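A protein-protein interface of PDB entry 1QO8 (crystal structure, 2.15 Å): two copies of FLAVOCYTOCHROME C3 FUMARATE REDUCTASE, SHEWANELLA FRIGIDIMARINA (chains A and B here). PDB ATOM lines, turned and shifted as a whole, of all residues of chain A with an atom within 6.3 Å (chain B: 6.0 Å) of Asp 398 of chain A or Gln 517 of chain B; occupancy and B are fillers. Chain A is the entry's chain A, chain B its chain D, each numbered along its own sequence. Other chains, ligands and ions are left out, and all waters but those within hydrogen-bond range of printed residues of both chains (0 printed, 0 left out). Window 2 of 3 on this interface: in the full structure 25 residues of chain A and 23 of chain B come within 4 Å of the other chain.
OG of Ser 518 of chain B lies within hydrogen-bond range of NH1 of Arg 196 of chain A. The side-chain amide nitrogen of Gln 517 of chain B lies close to the guanidinium group of Arg 196 of chain A (2.9 Å). NH1 of Arg 196 of chain A sits at hydrogen-bond distance from O of Leu 516 of chain B, at 3.0 Å.
OG of Ser 350 of chain B sits at hydrogen-bond distance from O of Asp 515 of chain B, at 2.8 Å. N of Gln 517 of chain B sits at hydrogen-bond distance from OD1 of Asp 515 of chain B (3.0 Å). OD1 of Asp 515 of chain B sits at hydrogen-bond distance from N of Ser 518 of chain B (3.1 Å).
Trp 356 of chain A touches Ser 350 of chain B (CZ2 to CB, 3.7 Å). Trp 356 of chain A touches Leu 516 of chain B. Ser 518 of chain B touches Trp 356 of chain A. OD2 of Asp 398 of chain A touches CD of Gln 517 of chain B (3.4 Å).
Of the printed residues of chain B, Arg 196 of chain A touches Leu 516 (3.0 Å), Gln 517 (2.9 Å) and Ser 518 (3.0 Å). Of the printed residues of chain B, Trp 356 of chain A touches Ser 350, Leu 516 and Ser 518. Of chain B, only Gln 517 comes within 4 Å of Asp 398 of chain A. Ala 403 of chain A touches none of the printed residues of chain B. Of the printed residues of chain A, Leu 516 of chain B touches Arg 196 (3.0 Å) and Trp 356 (3.4 Å). Gln 517 of chain B touches two residues of chain A. The nearest printed residue of chain B that does not touch Asp 398 of chain A is Asp 515 of chain B (7.1 Å).
Hydrophobic or aromatic side chains of chain A that line the printed part of chain B: Trp 356. Among the printed residues, 7 pairs touch across the chains. Among the printed residues, no Asp or Glu carboxylate lies within 4 Å of a Lys or Arg side-chain nitrogen of the other chain.
No position is printed for both chains. Of the 7 pairs that touch across the chains among the printed residues, none has its exchanged pair printed and touching as well.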
ATOM      1  N   ARG A 196      24.585  15.655  17.846  1.00  0.00           N
ATOM      2  CA  ARG A 196      24.689  14.628  18.878  1.00  0.00           C
ATOM      3  C   ARG A 196      25.936  13.771  18.811  1.00  0.00           C
ATOM      4  O   ARG A 196      25.927  12.592  19.191  1.00  0.00           O
ATOM      5  CB  ARG A 196      23.496  13.652  18.935  1.00  0.00           C
ATOM      6  CG  ARG A 196      22.153  14.378  19.053  1.00  0.00           C
ATOM      7  CD  ARG A 196      20.953  13.411  19.049  1.00  0.00           C
ATOM      8  NE  ARG A 196      19.766  14.233  18.732  1.00  0.00           N
ATOM      9  CZ  ARG A 196      18.634  13.724  18.326  1.00  0.00           C
ATOM     10  NH1 ARG A 196      18.554  12.367  18.216  1.00  0.00           N
ATOM     11  NH2 ARG A 196      17.556  14.482  18.030  1.00  0.00           N
ATOM     12  N   TRP A 356      17.822   9.852   9.136  1.00  0.00           N
ATOM     13  CA  TRP A 356      17.783  10.950  10.122  1.00  0.00           C
ATOM     14  C   TRP A 356      17.117  12.188   9.482  1.00  0.00           C
ATOM     15  O   TRP A 356      17.642  12.642   8.450  1.00  0.00           O
ATOM     16  CB  TRP A 356      19.152  11.268  10.776  1.00  0.00           C
ATOM     17  CG  TRP A 356      19.365  10.224  11.846  1.00  0.00           C
ATOM     18  CD1 TRP A 356      20.018   9.030  11.716  1.00  0.00           C
ATOM     19  CD2 TRP A 356      18.874  10.258  13.184  1.00  0.00           C
ATOM     20  NE1 TRP A 356      19.977   8.303  12.885  1.00  0.00           N
ATOM     21  CE2 TRP A 356      19.262   9.038  13.794  1.00  0.00           C
ATOM     22  CE3 TRP A 356      18.108  11.181  13.894  1.00  0.00           C
ATOM     23  CZ2 TRP A 356      18.906   8.730  15.113  1.00  0.00           C
ATOM     24  CZ3 TRP A 356      17.738  10.857  15.195  1.00  0.00           C
ATOM     25  CH2 TRP A 356      18.186   9.671  15.797  1.00  0.00           C
ATOM     26  N   PRO A 361       8.422  22.264  14.152  1.00  0.00           N
ATOM     27  CA  PRO A 361       7.150  22.188  14.783  1.00  0.00           C
ATOM     28  C   PRO A 361       5.949  22.853  14.229  1.00  0.00           C
ATOM     29  O   PRO A 361       4.833  22.370  14.434  1.00  0.00           O
ATOM     30  CB  PRO A 361       7.402  22.587  16.261  1.00  0.00           C
ATOM     31  CG  PRO A 361       8.714  23.237  16.234  1.00  0.00           C
ATOM     32  CD  PRO A 361       9.506  22.903  14.975  1.00  0.00           C
ATOM     33  N   THR A 396       9.123  22.582  24.605  1.00  0.00           N
ATOM     34  CA  THR A 396      10.222  22.389  23.668  1.00  0.00           C
ATOM     35  C   THR A 396       9.610  22.076  22.304  1.00  0.00           C
ATOM     36  O   THR A 396       8.474  21.593  22.217  1.00  0.00           O
ATOM     37  CB  THR A 396      11.093  21.157  24.054  1.00  0.00           C
ATOM     38  OG1 THR A 396      10.103  20.088  24.036  1.00  0.00           O
ATOM     39  CG2 THR A 396      11.622  21.191  25.495  1.00  0.00           C
ATOM     40  N   ARG A 397      10.463  22.065  21.282  1.00  0.00           N
ATOM     41  CA  ARG A 397       9.948  21.908  19.913  1.00  0.00           C
ATOM     42  C   ARG A 397       9.491  20.471  19.707  1.00  0.00           C
ATOM     43  O   ARG A 397       8.483  20.235  19.065  1.00  0.00           O
ATOM     44  CB  ARG A 397      11.016  22.209  18.879  1.00  0.00           C
ATOM     45  CG  ARG A 397      11.700  23.527  19.107  1.00  0.00           C
ATOM     46  CD  ARG A 397      12.984  23.505  18.283  1.00  0.00           C
ATOM     47  NE  ARG A 397      13.683  24.773  18.487  1.00  0.00           N
ATOM     48  CZ  ARG A 397      14.071  25.445  17.389  1.00  0.00           C
ATOM     49  NH1 ARG A 397      13.737  24.917  16.199  1.00  0.00           N
ATOM     50  NH2 ARG A 397      14.736  26.592  17.481  1.00  0.00           N
ATOM     51  N   ASP A 398      10.277  19.506  20.230  1.00  0.00           N
ATOM     52  CA  ASP A 398       9.819  18.131  19.957  1.00  0.00           C
ATOM     53  C   ASP A 398       8.540  17.820  20.691  1.00  0.00           C
ATOM     54  O   ASP A 398       7.754  17.064  20.194  1.00  0.00           O
ATOM     55  CB  ASP A 398      10.854  17.048  20.156  1.00  0.00           C
ATOM     56  CG  ASP A 398      11.698  17.170  21.376  1.00  0.00           C
ATOM     57  OD1 ASP A 398      11.191  16.850  22.473  1.00  0.00           O
ATOM     58  OD2 ASP A 398      12.889  17.572  21.189  1.00  0.00           O
ATOM     59  N   LYS A 399       8.317  18.284  21.927  1.00  0.00           N
ATOM     60  CA  LYS A 399       7.009  18.170  22.535  1.00  0.00           C
ATOM     61  C   LYS A 399       5.864  18.820  21.786  1.00  0.00           C
ATOM     62  O   LYS A 399       4.744  18.283  21.707  1.00  0.00           O
ATOM     63  CB  LYS A 399       7.098  18.745  23.971  1.00  0.00           C
ATOM     64  CG  LYS A 399       7.828  17.770  24.940  1.00  0.00           C
ATOM     65  CD  LYS A 399       7.662  18.300  26.356  1.00  0.00           C
ATOM     66  CE  LYS A 399       8.386  17.587  27.460  1.00  0.00           C
ATOM     67  NZ  LYS A 399       9.792  17.216  27.103  1.00  0.00           N
ATOM     68  N   ALA A 400       6.040  20.054  21.298  1.00  0.00           N
ATOM     69  CA  ALA A 400       5.052  20.712  20.492  1.00  0.00           C
ATOM     70  C   ALA A 400       4.800  19.914  19.225  1.00  0.00           C
ATOM     71  O   ALA A 400       3.602  19.630  18.987  1.00  0.00           O
ATOM     72  CB  ALA A 400       5.421  22.207  20.309  1.00  0.00           C
ATOM     73  N   SER A 401       5.726  19.418  18.441  1.00  0.00           N
ATOM     74  CA  SER A 401       5.332  18.590  17.279  1.00  0.00           C
ATOM     75  C   SER A 401       4.526  17.336  17.624  1.00  0.00           C
ATOM     76  O   SER A 401       3.519  17.074  16.992  1.00  0.00           O
ATOM     77  CB  SER A 401       6.542  17.892  16.545  1.00  0.00           C
ATOM     78  OG  SER A 401       7.403  19.008  16.454  1.00  0.00           O
ATOM     79  N   ASP A 402       5.046  16.637  18.655  1.00  0.00           N
ATOM     80  CA  ASP A 402       4.359  15.400  19.044  1.00  0.00           C
ATOM     81  C   ASP A 402       2.995  15.748  19.584  1.00  0.00           C
ATOM     82  O   ASP A 402       2.076  15.050  19.118  1.00  0.00           O
ATOM     83  CB  ASP A 402       5.161  14.562  20.074  1.00  0.00           C
ATOM     84  CG  ASP A 402       4.372  13.279  20.391  1.00  0.00           C
ATOM     85  OD1 ASP A 402       4.244  12.406  19.504  1.00  0.00           O
ATOM     86  OD2 ASP A 402       3.803  13.151  21.498  1.00  0.00           O
ATOM     87  N   ALA A 403       2.750  16.812  20.370  1.00  0.00           N
ATOM     88  CA  ALA A 403       1.343  17.033  20.763  1.00  0.00           C
ATOM     89  C   ALA A 403       0.460  17.524  19.621  1.00  0.00           C
ATOM     90  O   ALA A 403      -0.720  17.212  19.560  1.00  0.00           O
ATOM     91  CB  ALA A 403       1.263  18.043  21.917  1.00  0.00           C
ATOM     92  N   SER B 350      14.419   5.252  17.238  1.00  0.00           N
ATOM     93  CA  SER B 350      15.502   5.419  16.330  1.00  0.00           C
ATOM     94  C   SER B 350      16.296   4.122  16.177  1.00  0.00           C
ATOM     95  O   SER B 350      16.256   3.225  17.004  1.00  0.00           O
ATOM     96  CB  SER B 350      16.450   6.540  16.747  1.00  0.00           C
ATOM     97  OG  SER B 350      17.076   6.477  18.004  1.00  0.00           O
ATOM     98  N   ASP B 515      14.717   6.849  21.553  1.00  0.00           N
ATOM     99  CA  ASP B 515      13.657   7.422  20.725  1.00  0.00           C
ATOM    100  C   ASP B 515      14.291   8.349  19.656  1.00  0.00           C
ATOM    101  O   ASP B 515      15.508   8.287  19.360  1.00  0.00           O
ATOM    102  CB  ASP B 515      12.576   8.151  21.512  1.00  0.00           C
ATOM    103  CG  ASP B 515      13.159   9.348  22.275  1.00  0.00           C
ATOM    104  OD1 ASP B 515      14.320   9.757  22.109  1.00  0.00           O
ATOM    105  OD2 ASP B 515      12.362   9.862  23.099  1.00  0.00           O
ATOM    106  N   LEU B 516      13.471   9.196  19.057  1.00  0.00           N
ATOM    107  CA  LEU B 516      14.053  10.014  17.960  1.00  0.00           C
ATOM    108  C   LEU B 516      14.909  11.118  18.520  1.00  0.00           C
ATOM    109  O   LEU B 516      15.639  11.698  17.724  1.00  0.00           O
ATOM    110  CB  LEU B 516      12.961  10.611  17.075  1.00  0.00           C
ATOM    111  CG  LEU B 516      12.039   9.614  16.358  1.00  0.00           C
ATOM    112  CD1 LEU B 516      11.108  10.380  15.429  1.00  0.00           C
ATOM    113  CD2 LEU B 516      12.874   8.539  15.653  1.00  0.00           C
ATOM    114  N   GLN B 517      14.785  11.543  19.774  1.00  0.00           N
ATOM    115  CA  GLN B 517      15.719  12.496  20.346  1.00  0.00           C
ATOM    116  C   GLN B 517      16.929  11.789  20.916  1.00  0.00           C
ATOM    117  O   GLN B 517      17.791  12.365  21.556  1.00  0.00           O
ATOM    118  CB  GLN B 517      14.978  13.334  21.406  1.00  0.00           C
ATOM    119  CG  GLN B 517      13.692  14.050  20.901  1.00  0.00           C
ATOM    120  CD  GLN B 517      13.955  14.733  19.565  1.00  0.00           C
ATOM    121  OE1 GLN B 517      13.148  14.648  18.628  1.00  0.00           O
ATOM    122  NE2 GLN B 517      15.113  15.362  19.377  1.00  0.00           N
ATOM    123  N   SER B 518      17.042  10.482  20.721  1.00  0.00           N
ATOM    124  CA  SER B 518      18.102   9.613  21.179  1.00  0.00           C
ATOM    125  C   SER B 518      18.028   9.417  22.714  1.00  0.00           C
ATOM    126  O   SER B 518      19.019   9.328  23.348  1.00  0.00           O
ATOM    127  CB  SER B 518      19.488  10.067  20.779  1.00  0.00           C
ATOM    128  OG  SER B 518      19.688   9.907  19.386  1.00  0.00           O
ATOM    129  N   LYS B 519      16.858   9.430  23.294  1.00  0.00           N
ATOM    130  CA  LYS B 519      16.555   9.281  24.678  1.00  0.00           C
ATOM    131  C   LYS B 519      15.867   7.951  24.951  1.00  0.00           C
ATOM    132  O   LYS B 519      15.072   7.547  24.123  1.00  0.00           O
ATOM    133  CB  LYS B 519      15.510  10.294  25.148  1.00  0.00           C
ATOM    134  CG  LYS B 519      15.876  11.737  24.981  1.00  0.00           C
ATOM    135  CD  LYS B 519      17.057  12.187  25.823  1.00  0.00           C
ATOM    136  CE  LYS B 519      16.810  13.673  26.121  1.00  0.00           C
ATOM    137  NZ  LYS B 519      18.103  14.372  26.432  1.00  0.00           N
